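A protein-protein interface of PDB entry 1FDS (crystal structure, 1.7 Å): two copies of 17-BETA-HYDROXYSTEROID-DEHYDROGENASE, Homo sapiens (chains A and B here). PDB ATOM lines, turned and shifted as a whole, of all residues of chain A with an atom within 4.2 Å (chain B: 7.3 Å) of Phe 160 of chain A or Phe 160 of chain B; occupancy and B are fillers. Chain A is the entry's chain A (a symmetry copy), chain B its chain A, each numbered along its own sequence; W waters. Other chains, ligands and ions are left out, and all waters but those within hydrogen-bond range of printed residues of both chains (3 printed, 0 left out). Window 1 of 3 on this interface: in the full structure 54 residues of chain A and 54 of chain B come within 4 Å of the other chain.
Among the printed residues, merely in contact across the chains: Met 147 of chain A with Glu 167 of chain B, Gly 148 of chain A with Ser 168 of chain B, Ala 157 of chain A with Ala 161 of chain B, Phe 160 of chain A with Phe 160 of chain B, Phe 160 of chain A with Glu 163 of chain B, Phe 160 of chain A with Gly 164 of chain B, Ala 161 of chain A with Ala 157 of chain B, Ala 161 of chain A with Ala 161 of chain B, Glu 163 of chain A with Phe 160 of chain B and Gly 164 of chain A with Phe 160 of chain B.
The guanidinium group (NH2) of Arg 266 of chain A sits close to the guanidinium group (NH2) of Arg 252 of chain B (3.5 Å).
The side-chain carboxylate (OE2) of Glu 167 of chain B is in hydrogen-bond range of the backbone NH (N) of Gly 148 of chain A.
OG of Ser 168 of chain B sits close to SG of Cys 156 of chain A (3.6 Å).
The guanidinium group (NE) of Arg 266 of chain A lies within salt-bridge range of the side-chain carboxylate (OE2) of Glu 167 of chain B (2.8 Å).
Printed residues of chain A that touch a printed residue of chain B: Met 147, Gly 148, Cys 156, Ala 157, Phe 160, Ala 161, Glu 163, Gly 164 and Arg 266.
Hydrophobic or aromatic side chains of chain A within 4 Å of the printed part of chain B: Ala 157, Phe 160 and Ala 161.
Hydrophobic or aromatic side chains of chain B within 4 Å of the printed part of chain A: Ala 157, Phe 160 and Ala 161.
Among the printed residues, Asp or Glu carboxylates within 4 Å of a Lys or Arg side-chain nitrogen of the other chain: Arg 266 of chain A with Glu 167 of chain B.
Phe 160 of chain A touches just these residues of chain B: Phe 160 (3.2 Å), Glu 163 (3.9 Å) and Gly 164 (3.5 Å).
Of chain A, only Phe 160 (3.2 Å), Glu 163 (3.9 Å) and Gly 164 (3.5 Å) come within 4 Å of Phe 160 of chain B.
Printed residues of chain B within 4 Å of Met 147 of chain A: Glu 167.
Of the printed residues of chain A, Glu 163 of chain B touches Phe 160.
Phe 160 of chain B touches its own counterpart, Phe 160 of chain A.
Phe 160 of chain A touches Glu 163 of chain B, and with the chains exchanged Glu 163 of chain A touches Phe 160 of chain B.
Phe 160 of chain A touches Gly 164 of chain B, and with the chains exchanged Gly 164 of chain A touches Phe 160 of chain B.
Ala 161 of chain A touches its own counterpart, Ala 161 of chain B.
15 positions are printed for both chains.
Of the 14 pairs that touch across the chains among the printed residues, 8 have their exchanged pair printed and touching as well.
Water W2 bridges the backbone carbonyl oxygen of Arg 266 of chain A (2.7 Å) and the guanidinium group of Arg 252 of chain B (3.2 Å).
Water W1 lies within hydrogen-bond range of the guanidinium group of Arg 266 of chain A (2.9 Å), the side-chain carboxylate of Glu 163 of chain B (3.0 Å) and the guanidinium group of Arg 252 of chain B (3.5 Å).
Water W3 bridges the guanidinium group (NH2) of Arg 266 of chain B and the side-chain carboxylate (OE1) of Glu 163 of chain A.
SG of Cys 156 of chain A lies close to O of Gly 144 of chain A, at 3.4 Å.
The backbone carbonyl oxygen of Leu 146 of chain A is in hydrogen-bond range of the guanidinium group of Arg 266 of chain A.
The side-chain carboxylate of Glu 163 of chain B lies within salt-bridge range of the guanidinium group of Arg 252 of chain B (2.7 Å).
The side-chain hydroxyl of Ser 168 of chain B sits at hydrogen-bond distance from the backbone carbonyl oxygen of Gly 164 of chain B (2.8 Å).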
ATOM      1  N   GLY A 144      17.206 -19.381   2.495  1.00  0.00           N
ATOM      2  CA  GLY A 144      16.769 -18.045   2.110  1.00  0.00           C
ATOM      3  C   GLY A 144      17.915 -17.025   2.217  1.00  0.00           C
ATOM      4  O   GLY A 144      17.743 -15.852   1.882  1.00  0.00           O
ATOM      5  N   GLY A 145      19.050 -17.437   2.772  1.00  0.00           N
ATOM      6  CA  GLY A 145      20.197 -16.552   2.833  1.00  0.00           C
ATOM      7  C   GLY A 145      21.096 -16.854   1.644  1.00  0.00           C
ATOM      8  O   GLY A 145      22.077 -16.157   1.402  1.00  0.00           O
ATOM      9  N   LEU A 146      20.731 -17.884   0.880  1.00  0.00           N
ATOM     10  CA  LEU A 146      21.510 -18.328  -0.285  1.00  0.00           C
ATOM     11  C   LEU A 146      20.860 -18.049  -1.629  1.00  0.00           C
ATOM     12  O   LEU A 146      21.542 -18.102  -2.663  1.00  0.00           O
ATOM     13  CB  LEU A 146      21.816 -19.832  -0.159  1.00  0.00           C
ATOM     14  CG  LEU A 146      22.585 -20.242   1.111  1.00  0.00           C
ATOM     15  CD1 LEU A 146      22.685 -21.756   1.161  1.00  0.00           C
ATOM     16  CD2 LEU A 146      23.960 -19.624   1.147  1.00  0.00           C
ATOM     17  N   MET A 147      19.548 -17.835  -1.618  1.00  0.00           N
ATOM     18  CA  MET A 147      18.794 -17.533  -2.817  1.00  0.00           C
ATOM     19  C   MET A 147      17.567 -16.740  -2.426  1.00  0.00           C
ATOM     20  O   MET A 147      16.983 -16.966  -1.361  1.00  0.00           O
ATOM     21  CB  MET A 147      18.398 -18.812  -3.551  1.00  0.00           C
ATOM     22  CG  MET A 147      17.575 -19.769  -2.719  1.00  0.00           C
ATOM     23  SD  MET A 147      17.449 -21.413  -3.506  1.00  0.00           S
ATOM     24  CE  MET A 147      15.732 -21.655  -3.180  1.00  0.00           C
ATOM     25  N   GLY A 148      17.189 -15.800  -3.291  1.00  0.00           N
ATOM     26  CA  GLY A 148      16.033 -14.949  -3.040  1.00  0.00           C
ATOM     27  C   GLY A 148      14.704 -15.669  -3.248  1.00  0.00           C
ATOM     28  O   GLY A 148      14.564 -16.472  -4.164  1.00  0.00           O
ATOM     29  N   CYS A 156      14.949 -12.621   3.470  1.00  0.00           N
ATOM     30  CA  CYS A 156      16.114 -13.007   2.665  1.00  0.00           C
ATOM     31  C   CYS A 156      17.204 -11.954   2.801  1.00  0.00           C
ATOM     32  O   CYS A 156      18.367 -12.297   2.932  1.00  0.00           O
ATOM     33  CB  CYS A 156      15.737 -13.181   1.194  1.00  0.00           C
ATOM     34  SG  CYS A 156      14.705 -14.650   0.960  1.00  0.00           S
ATOM     35  N   ALA A 157      16.835 -10.679   2.790  1.00  0.00           N
ATOM     36  CA  ALA A 157      17.835  -9.625   2.967  1.00  0.00           C
ATOM     37  C   ALA A 157      18.598  -9.885   4.257  1.00  0.00           C
ATOM     38  O   ALA A 157      19.834  -9.889   4.273  1.00  0.00           O
ATOM     39  CB  ALA A 157      17.182  -8.226   3.020  1.00  0.00           C
ATOM     40  N   SER A 158      17.875 -10.171   5.334  1.00  0.00           N
ATOM     41  CA  SER A 158      18.510 -10.408   6.629  1.00  0.00           C
ATOM     42  C   SER A 158      19.382 -11.675   6.668  1.00  0.00           C
ATOM     43  O   SER A 158      20.443 -11.668   7.294  1.00  0.00           O
ATOM     44  CB  SER A 158      17.447 -10.399   7.758  1.00  0.00           C
ATOM     45  OG  SER A 158      16.822 -11.649   7.891  1.00  0.00           O
ATOM     46  N   LYS A 159      18.948 -12.765   6.020  1.00  0.00           N
ATOM     47  CA  LYS A 159      19.720 -14.004   6.011  1.00  0.00           C
ATOM     48  C   LYS A 159      20.938 -13.886   5.082  1.00  0.00           C
ATOM     49  O   LYS A 159      22.015 -14.407   5.399  1.00  0.00           O
ATOM     50  CB  LYS A 159      18.816 -15.205   5.688  1.00  0.00           C
ATOM     51  CG  LYS A 159      17.795 -15.465   6.820  1.00  0.00           C
ATOM     52  CD  LYS A 159      18.524 -15.970   8.059  1.00  0.00           C
ATOM     53  CE  LYS A 159      17.646 -16.026   9.271  1.00  0.00           C
ATOM     54  NZ  LYS A 159      18.418 -16.707  10.379  1.00  0.00           N
ATOM     55  N   PHE A 160      20.792 -13.169   3.960  1.00  0.00           N
ATOM     56  CA  PHE A 160      21.936 -12.926   3.076  1.00  0.00           C
ATOM     57  C   PHE A 160      22.953 -12.090   3.863  1.00  0.00           C
ATOM     58  O   PHE A 160      24.162 -12.306   3.760  1.00  0.00           O
ATOM     59  CB  PHE A 160      21.526 -12.116   1.855  1.00  0.00           C
ATOM     60  CG  PHE A 160      21.177 -12.947   0.669  1.00  0.00           C
ATOM     61  CD1 PHE A 160      20.003 -13.715   0.647  1.00  0.00           C
ATOM     62  CD2 PHE A 160      21.993 -12.918  -0.454  1.00  0.00           C
ATOM     63  CE1 PHE A 160      19.653 -14.433  -0.503  1.00  0.00           C
ATOM     64  CE2 PHE A 160      21.644 -13.632  -1.598  1.00  0.00           C
ATOM     65  CZ  PHE A 160      20.467 -14.387  -1.618  1.00  0.00           C
ATOM     66  N   ALA A 161      22.454 -11.127   4.625  1.00  0.00           N
ATOM     67  CA  ALA A 161      23.321 -10.255   5.429  1.00  0.00           C
ATOM     68  C   ALA A 161      24.192 -11.081   6.360  1.00  0.00           C
ATOM     69  O   ALA A 161      25.384 -10.812   6.490  1.00  0.00           O
ATOM     70  CB  ALA A 161      22.482  -9.243   6.231  1.00  0.00           C
ATOM     71  N   LEU A 162      23.616 -12.113   6.969  1.00  0.00           N
ATOM     72  CA  LEU A 162      24.368 -12.991   7.863  1.00  0.00           C
ATOM     73  C   LEU A 162      25.446 -13.726   7.102  1.00  0.00           C
ATOM     74  O   LEU A 162      26.526 -13.938   7.634  1.00  0.00           O
ATOM     75  CB  LEU A 162      23.449 -14.006   8.570  1.00  0.00           C
ATOM     76  CG  LEU A 162      22.471 -13.494   9.634  1.00  0.00           C
ATOM     77  CD1 LEU A 162      21.739 -14.704  10.236  1.00  0.00           C
ATOM     78  CD2 LEU A 162      23.232 -12.751  10.721  1.00  0.00           C
ATOM     79  N   GLU A 163      25.171 -14.098   5.852  1.00  0.00           N
ATOM     80  CA  GLU A 163      26.164 -14.805   5.048  1.00  0.00           C
ATOM     81  C   GLU A 163      27.373 -13.884   4.871  1.00  0.00           C
ATOM     82  O   GLU A 163      28.514 -14.299   5.085  1.00  0.00           O
ATOM     83  CB  GLU A 163      25.611 -15.153   3.666  1.00  0.00           C
ATOM     84  CG  GLU A 163      24.499 -16.190   3.673  1.00  0.00           C
ATOM     85  CD  GLU A 163      24.968 -17.571   4.034  1.00  0.00           C
ATOM     86  OE1 GLU A 163      26.045 -17.996   3.579  1.00  0.00           O
ATOM     87  OE2 GLU A 163      24.227 -18.267   4.746  1.00  0.00           O
ATOM     88  N   GLY A 164      27.118 -12.634   4.491  1.00  0.00           N
ATOM     89  CA  GLY A 164      28.211 -11.701   4.267  1.00  0.00           C
ATOM     90  C   GLY A 164      28.977 -11.421   5.539  1.00  0.00           C
ATOM     91  O   GLY A 164      30.201 -11.373   5.544  1.00  0.00           O
ATOM     92  N   ARG A 266      21.881 -21.152  -9.722  1.00  0.00           N
ATOM     93  CA  ARG A 266      22.011 -19.780  -9.285  1.00  0.00           C
ATOM     94  C   ARG A 266      23.481 -19.377  -9.402  1.00  0.00           C
ATOM     95  O   ARG A 266      23.813 -18.317  -9.935  1.00  0.00           O
ATOM     96  CB  ARG A 266      21.543 -19.675  -7.839  1.00  0.00           C
ATOM     97  CG  ARG A 266      21.511 -18.286  -7.395  1.00  0.00           C
ATOM     98  CD  ARG A 266      21.164 -18.168  -5.971  1.00  0.00           C
ATOM     99  NE  ARG A 266      21.211 -16.756  -5.686  1.00  0.00           N
ATOM    100  CZ  ARG A 266      22.309 -16.091  -5.360  1.00  0.00           C
ATOM    101  NH1 ARG A 266      23.471 -16.720  -5.235  1.00  0.00           N
ATOM    102  NH2 ARG A 266      22.278 -14.770  -5.277  1.00  0.00           N
ATOM    103  N   VAL B 115      20.411  -0.677   3.532  1.00  0.00           N
ATOM    104  CA  VAL B 115      19.345  -1.637   3.345  1.00  0.00           C
ATOM    105  C   VAL B 115      17.956  -1.073   3.564  1.00  0.00           C
ATOM    106  O   VAL B 115      17.154  -1.073   2.630  1.00  0.00           O
ATOM    107  CB  VAL B 115      19.568  -2.899   4.215  1.00  0.00           C
ATOM    108  CG1 VAL B 115      18.567  -3.970   3.835  1.00  0.00           C
ATOM    109  CG2 VAL B 115      20.986  -3.412   4.021  1.00  0.00           C
ATOM    110  N   SER B 142      27.973  -4.308  -5.166  1.00  0.00           N
ATOM    111  CA  SER B 142      29.416  -4.333  -4.963  1.00  0.00           C
ATOM    112  C   SER B 142      29.854  -5.769  -4.996  1.00  0.00           C
ATOM    113  O   SER B 142      29.054  -6.668  -4.744  1.00  0.00           O
ATOM    114  CB  SER B 142      29.750  -3.743  -3.574  1.00  0.00           C
ATOM    115  OG  SER B 142      31.064  -4.066  -3.137  1.00  0.00           O
ATOM    116  N   VAL B 143      31.102  -5.997  -5.369  1.00  0.00           N
ATOM    117  CA  VAL B 143      31.619  -7.362  -5.335  1.00  0.00           C
ATOM    118  C   VAL B 143      31.592  -7.805  -3.834  1.00  0.00           C
ATOM    119  O   VAL B 143      31.549  -8.987  -3.553  1.00  0.00           O
ATOM    120  CB  VAL B 143      33.043  -7.443  -5.922  1.00  0.00           C
ATOM    121  CG1 VAL B 143      33.925  -6.564  -5.176  1.00  0.00           C
ATOM    122  CG2 VAL B 143      33.580  -8.881  -5.846  1.00  0.00           C
ATOM    123  N   GLY B 144      31.563  -6.843  -2.906  1.00  0.00           N
ATOM    124  CA  GLY B 144      31.465  -7.118  -1.477  1.00  0.00           C
ATOM    125  C   GLY B 144      30.070  -7.644  -1.099  1.00  0.00           C
ATOM    126  O   GLY B 144      29.820  -7.979   0.060  1.00  0.00           O
ATOM    127  N   GLY B 145      29.134  -7.627  -2.043  1.00  0.00           N
ATOM    128  CA  GLY B 145      27.820  -8.182  -1.779  1.00  0.00           C
ATOM    129  C   GLY B 145      27.794  -9.612  -2.292  1.00  0.00           C
ATOM    130  O   GLY B 145      26.830 -10.341  -2.081  1.00  0.00           O
ATOM    131  N   LEU B 146      28.885 -10.022  -2.942  1.00  0.00           N
ATOM    132  CA  LEU B 146      29.005 -11.363  -3.531  1.00  0.00           C
ATOM    133  C   LEU B 146      29.979 -12.286  -2.820  1.00  0.00           C
ATOM    134  O   LEU B 146      29.938 -13.506  -3.037  1.00  0.00           O
ATOM    135  CB  LEU B 146      29.396 -11.242  -5.016  1.00  0.00           C
ATOM    136  CG  LEU B 146      28.422 -10.426  -5.888  1.00  0.00           C
ATOM    137  CD1 LEU B 146      29.010 -10.277  -7.279  1.00  0.00           C
ATOM    138  CD2 LEU B 146      27.064 -11.079  -5.958  1.00  0.00           C
ATOM    139  N   MET B 147      30.889 -11.702  -2.046  1.00  0.00           N
ATOM    140  CA  MET B 147      31.868 -12.451  -1.287  1.00  0.00           C
ATOM    141  C   MET B 147      32.280 -11.626  -0.088  1.00  0.00           C
ATOM    142  O   MET B 147      32.358 -10.395  -0.166  1.00  0.00           O
ATOM    143  CB  MET B 147      33.082 -12.794  -2.148  1.00  0.00           C
ATOM    144  CG  MET B 147      33.780 -11.590  -2.735  1.00  0.00           C
ATOM    145  SD  MET B 147      34.975 -12.067  -4.033  1.00  0.00           S
ATOM    146  CE  MET B 147      36.263 -10.975  -3.524  1.00  0.00           C
ATOM    147  N   GLY B 148      32.531 -12.312   1.026  1.00  0.00           N
ATOM    148  CA  GLY B 148      32.924 -11.650   2.262  1.00  0.00           C
ATOM    149  C   GLY B 148      34.369 -11.159   2.244  1.00  0.00           C
ATOM    150  O   GLY B 148      35.250 -11.828   1.715  1.00  0.00           O
ATOM    151  N   LEU B 149      34.607  -9.973   2.789  1.00  0.00           N
ATOM    152  CA  LEU B 149      35.950  -9.360   2.814  1.00  0.00           C
ATOM    153  C   LEU B 149      36.288  -9.064   4.265  1.00  0.00           C
ATOM    154  O   LEU B 149      35.507  -8.423   4.961  1.00  0.00           O
ATOM    155  CB  LEU B 149      35.946  -8.063   2.022  1.00  0.00           C
ATOM    156  CG  LEU B 149      35.508  -8.197   0.563  1.00  0.00           C
ATOM    157  CD1 LEU B 149      35.209  -6.823  -0.044  1.00  0.00           C
ATOM    158  CD2 LEU B 149      36.595  -8.951  -0.184  1.00  0.00           C
ATOM    159  N   ASP B 153      32.979  -6.577   7.440  1.00  0.00           N
ATOM    160  CA  ASP B 153      31.853  -7.400   7.876  1.00  0.00           C
ATOM    161  C   ASP B 153      30.482  -6.758   7.721  1.00  0.00           C
ATOM    162  O   ASP B 153      29.581  -7.362   7.152  1.00  0.00           O
ATOM    163  CB  ASP B 153      32.032  -7.819   9.344  1.00  0.00           C
ATOM    164  CG  ASP B 153      33.475  -8.205   9.687  1.00  0.00           C
ATOM    165  OD1 ASP B 153      34.008  -9.197   9.183  1.00  0.00           O
ATOM    166  OD2 ASP B 153      34.053  -7.507  10.506  1.00  0.00           O
ATOM    167  N   VAL B 154      30.328  -5.546   8.241  1.00  0.00           N
ATOM    168  CA  VAL B 154      29.042  -4.857   8.213  1.00  0.00           C
ATOM    169  C   VAL B 154      28.728  -4.307   6.836  1.00  0.00           C
ATOM    170  O   VAL B 154      27.593  -4.359   6.400  1.00  0.00           O
ATOM    171  CB  VAL B 154      28.964  -3.767   9.291  1.00  0.00           C
ATOM    172  CG1 VAL B 154      27.581  -3.071   9.247  1.00  0.00           C
ATOM    173  CG2 VAL B 154      29.215  -4.401  10.677  1.00  0.00           C
ATOM    174  N   TYR B 155      29.741  -3.805   6.135  1.00  0.00           N
ATOM    175  CA  TYR B 155      29.540  -3.319   4.780  1.00  0.00           C
ATOM    176  C   TYR B 155      29.071  -4.501   3.907  1.00  0.00           C
ATOM    177  O   TYR B 155      28.109  -4.376   3.162  1.00  0.00           O
ATOM    178  CB  TYR B 155      30.849  -2.763   4.220  1.00  0.00           C
ATOM    179  CG  TYR B 155      30.722  -2.350   2.770  1.00  0.00           C
ATOM    180  CD1 TYR B 155      29.995  -1.217   2.406  1.00  0.00           C
ATOM    181  CD2 TYR B 155      31.336  -3.091   1.765  1.00  0.00           C
ATOM    182  CE1 TYR B 155      29.895  -0.829   1.068  1.00  0.00           C
ATOM    183  CE2 TYR B 155      31.241  -2.716   0.431  1.00  0.00           C
ATOM    184  CZ  TYR B 155      30.526  -1.585   0.090  1.00  0.00           C
ATOM    185  OH  TYR B 155      30.467  -1.201  -1.226  1.00  0.00           O
ATOM    186  N   CYS B 156      29.799  -5.622   3.960  1.00  0.00           N
ATOM    187  CA  CYS B 156      29.435  -6.826   3.204  1.00  0.00           C
ATOM    188  C   CYS B 156      28.056  -7.304   3.632  1.00  0.00           C
ATOM    189  O   CYS B 156      27.256  -7.683   2.793  1.00  0.00           O
ATOM    190  CB  CYS B 156      30.461  -7.941   3.409  1.00  0.00           C
ATOM    191  SG  CYS B 156      32.029  -7.534   2.599  1.00  0.00           S
ATOM    192  N   ALA B 157      27.766  -7.272   4.928  1.00  0.00           N
ATOM    193  CA  ALA B 157      26.438  -7.673   5.392  1.00  0.00           C
ATOM    194  C   ALA B 157      25.392  -6.852   4.653  1.00  0.00           C
ATOM    195  O   ALA B 157      24.433  -7.399   4.096  1.00  0.00           O
ATOM    196  CB  ALA B 157      26.282  -7.469   6.915  1.00  0.00           C
ATOM    197  N   SER B 158      25.599  -5.542   4.583  1.00  0.00           N
ATOM    198  CA  SER B 158      24.639  -4.661   3.921  1.00  0.00           C
ATOM    199  C   SER B 158      24.524  -4.897   2.405  1.00  0.00           C
ATOM    200  O   SER B 158      23.424  -4.825   1.856  1.00  0.00           O
ATOM    201  CB  SER B 158      24.952  -3.179   4.257  1.00  0.00           C
ATOM    202  OG  SER B 158      25.942  -2.654   3.411  1.00  0.00           O
ATOM    203  N   LYS B 159      25.643  -5.166   1.718  1.00  0.00           N
ATOM    204  CA  LYS B 159      25.614  -5.402   0.277  1.00  0.00           C
ATOM    205  C   LYS B 159      25.035  -6.789  -0.040  1.00  0.00           C
ATOM    206  O   LYS B 159      24.300  -6.946  -1.024  1.00  0.00           O
ATOM    207  CB  LYS B 159      27.000  -5.159  -0.340  1.00  0.00           C
ATOM    208  CG  LYS B 159      27.401  -3.667  -0.263  1.00  0.00           C
ATOM    209  CD  LYS B 159      26.515  -2.851  -1.196  1.00  0.00           C
ATOM    210  CE  LYS B 159      26.678  -1.374  -1.012  1.00  0.00           C
ATOM    211  NZ  LYS B 159      25.897  -0.677  -2.103  1.00  0.00           N
ATOM    212  N   PHE B 160      25.323  -7.787   0.806  1.00  0.00           N
ATOM    213  CA  PHE B 160      24.724  -9.113   0.625  1.00  0.00           C
ATOM    214  C   PHE B 160      23.210  -8.961   0.809  1.00  0.00           C
ATOM    215  O   PHE B 160      22.421  -9.579   0.093  1.00  0.00           O
ATOM    216  CB  PHE B 160      25.218 -10.088   1.684  1.00  0.00           C
ATOM    217  CG  PHE B 160      26.394 -10.898   1.258  1.00  0.00           C
ATOM    218  CD1 PHE B 160      27.657 -10.309   1.105  1.00  0.00           C
ATOM    219  CD2 PHE B 160      26.252 -12.266   1.066  1.00  0.00           C
ATOM    220  CE1 PHE B 160      28.766 -11.098   0.775  1.00  0.00           C
ATOM    221  CE2 PHE B 160      27.355 -13.050   0.737  1.00  0.00           C
ATOM    222  CZ  PHE B 160      28.615 -12.458   0.597  1.00  0.00           C
ATOM    223  N   ALA B 161      22.817  -8.154   1.785  1.00  0.00           N
ATOM    224  CA  ALA B 161      21.394  -7.922   2.067  1.00  0.00           C
ATOM    225  C   ALA B 161      20.682  -7.411   0.826  1.00  0.00           C
ATOM    226  O   ALA B 161      19.582  -7.864   0.515  1.00  0.00           O
ATOM    227  CB  ALA B 161      21.224  -6.931   3.233  1.00  0.00           C
ATOM    228  N   LEU B 162      21.324  -6.509   0.090  1.00  0.00           N
ATOM    229  CA  LEU B 162      20.743  -5.972  -1.140  1.00  0.00           C
ATOM    230  C   LEU B 162      20.585  -7.063  -2.172  1.00  0.00           C
ATOM    231  O   LEU B 162      19.611  -7.061  -2.911  1.00  0.00           O
ATOM    232  CB  LEU B 162      21.597  -4.829  -1.720  1.00  0.00           C
ATOM    233  CG  LEU B 162      21.645  -3.493  -0.969  1.00  0.00           C
ATOM    234  CD1 LEU B 162      22.490  -2.508  -1.793  1.00  0.00           C
ATOM    235  CD2 LEU B 162      20.235  -2.950  -0.792  1.00  0.00           C
ATOM    236  N   GLU B 163      21.523  -8.009  -2.216  1.00  0.00           N
ATOM    237  CA  GLU B 163      21.437  -9.102  -3.182  1.00  0.00           C
ATOM    238  C   GLU B 163      20.166  -9.898  -2.882  1.00  0.00           C
ATOM    239  O   GLU B 163      19.378 -10.185  -3.786  1.00  0.00           O
ATOM    240  CB  GLU B 163      22.638 -10.040  -3.063  1.00  0.00           C
ATOM    241  CG  GLU B 163      23.963  -9.427  -3.486  1.00  0.00           C
ATOM    242  CD  GLU B 163      24.068  -9.183  -4.965  1.00  0.00           C
ATOM    243  OE1 GLU B 163      23.633 -10.033  -5.763  1.00  0.00           O
ATOM    244  OE2 GLU B 163      24.638  -8.148  -5.343  1.00  0.00           O
ATOM    245  N   GLY B 164      19.964 -10.242  -1.612  1.00  0.00           N
ATOM    246  CA  GLY B 164      18.797 -11.029  -1.244  1.00  0.00           C
ATOM    247  C   GLY B 164      17.511 -10.278  -1.503  1.00  0.00           C
ATOM    248  O   GLY B 164      16.544 -10.834  -2.007  1.00  0.00           O
ATOM    249  N   LEU B 165      17.499  -9.001  -1.159  1.00  0.00           N
ATOM    250  CA  LEU B 165      16.324  -8.175  -1.345  1.00  0.00           C
ATOM    251  C   LEU B 165      15.929  -8.098  -2.815  1.00  0.00           C
ATOM    252  O   LEU B 165      14.783  -8.338  -3.188  1.00  0.00           O
ATOM    253  CB  LEU B 165      16.608  -6.766  -0.822  1.00  0.00           C
ATOM    254  CG  LEU B 165      15.493  -5.738  -1.035  1.00  0.00           C
ATOM    255  CD1 LEU B 165      14.459  -5.975   0.055  1.00  0.00           C
ATOM    256  CD2 LEU B 165      16.054  -4.301  -0.881  1.00  0.00           C
ATOM    257  N   CYS B 166      16.888  -7.734  -3.648  1.00  0.00           N
ATOM    258  CA  CYS B 166      16.666  -7.570  -5.066  1.00  0.00           C
ATOM    259  C   CYS B 166      16.313  -8.856  -5.787  1.00  0.00           C
ATOM    260  O   CYS B 166      15.438  -8.843  -6.645  1.00  0.00           O
ATOM    261  CB  CYS B 166      17.882  -6.911  -5.706  1.00  0.00           C
ATOM    262  SG  CYS B 166      18.025  -5.207  -5.178  1.00  0.00           S
ATOM    263  N   GLU B 167      16.985  -9.949  -5.448  1.00  0.00           N
ATOM    264  CA  GLU B 167      16.711 -11.227  -6.078  1.00  0.00           C
ATOM    265  C   GLU B 167      15.290 -11.696  -5.761  1.00  0.00           C
ATOM    266  O   GLU B 167      14.573 -12.163  -6.641  1.00  0.00           O
ATOM    267  CB  GLU B 167      17.728 -12.254  -5.610  1.00  0.00           C
ATOM    268  CG  GLU B 167      17.759 -13.458  -6.487  1.00  0.00           C
ATOM    269  CD  GLU B 167      18.982 -14.285  -6.230  1.00  0.00           C
ATOM    270  OE1 GLU B 167      20.054 -13.972  -6.761  1.00  0.00           O
ATOM    271  OE2 GLU B 167      18.874 -15.257  -5.482  1.00  0.00           O
ATOM    272  N   SER B 168      14.870 -11.520  -4.517  1.00  0.00           N
ATOM    273  CA  SER B 168      13.528 -11.877  -4.082  1.00  0.00           C
ATOM    274  C   SER B 168      12.498 -11.068  -4.878  1.00  0.00           C
ATOM    275  O   SER B 168      11.513 -11.611  -5.374  1.00  0.00           O
ATOM    276  CB  SER B 168      13.389 -11.591  -2.588  1.00  0.00           C
ATOM    277  OG  SER B 168      14.288 -12.399  -1.845  1.00  0.00           O
ATOM    278  N   ARG B 252      21.849  -8.958 -12.785  1.00  0.00           N
ATOM    279  CA  ARG B 252      23.143  -8.382 -12.425  1.00  0.00           C
ATOM    280  C   ARG B 252      23.983  -8.011 -13.616  1.00  0.00           C
ATOM    281  O   ARG B 252      24.038  -8.759 -14.607  1.00  0.00           O
ATOM    282  CB  ARG B 252      23.990  -9.374 -11.648  1.00  0.00           C
ATOM    283  CG  ARG B 252      23.437  -9.745 -10.361  1.00  0.00           C
ATOM    284  CD  ARG B 252      24.398 -10.624  -9.580  1.00  0.00           C
ATOM    285  NE  ARG B 252      23.694 -10.921  -8.359  1.00  0.00           N
ATOM    286  CZ  ARG B 252      22.783 -11.864  -8.240  1.00  0.00           C
ATOM    287  NH1 ARG B 252      22.501 -12.659  -9.280  1.00  0.00           N
ATOM    288  NH2 ARG B 252      21.993 -11.854  -7.179  1.00  0.00           N
ATOM    289  N   ARG B 266      34.210 -19.609  -4.971  1.00  0.00           N
ATOM    290  CA  ARG B 266      33.292 -19.417  -3.871  1.00  0.00           C
ATOM    291  C   ARG B 266      32.028 -20.228  -4.154  1.00  0.00           C
ATOM    292  O   ARG B 266      31.528 -20.955  -3.294  1.00  0.00           O
ATOM    293  CB  ARG B 266      32.960 -17.934  -3.757  1.00  0.00           C
ATOM    294  CG  ARG B 266      32.156 -17.664  -2.571  1.00  0.00           C
ATOM    295  CD  ARG B 266      31.735 -16.257  -2.496  1.00  0.00           C
ATOM    296  NE  ARG B 266      30.931 -16.166  -1.304  1.00  0.00           N
ATOM    297  CZ  ARG B 266      29.637 -16.441  -1.247  1.00  0.00           C
ATOM    298  NH1 ARG B 266      28.970 -16.796  -2.339  1.00  0.00           N
ATOM    299  NH2 ARG B 266      29.024 -16.484  -0.074  1.00  0.00           N
HETATM  300  O   HOH W   1      24.280 -12.734  -4.740  1.00  0.00           O
HETATM  301  O   HOH W   2      23.434 -15.693  -9.347  1.00  0.00           O
HETATM  302  O   HOH W   3      26.316 -17.118   0.766  1.00  0.00           O
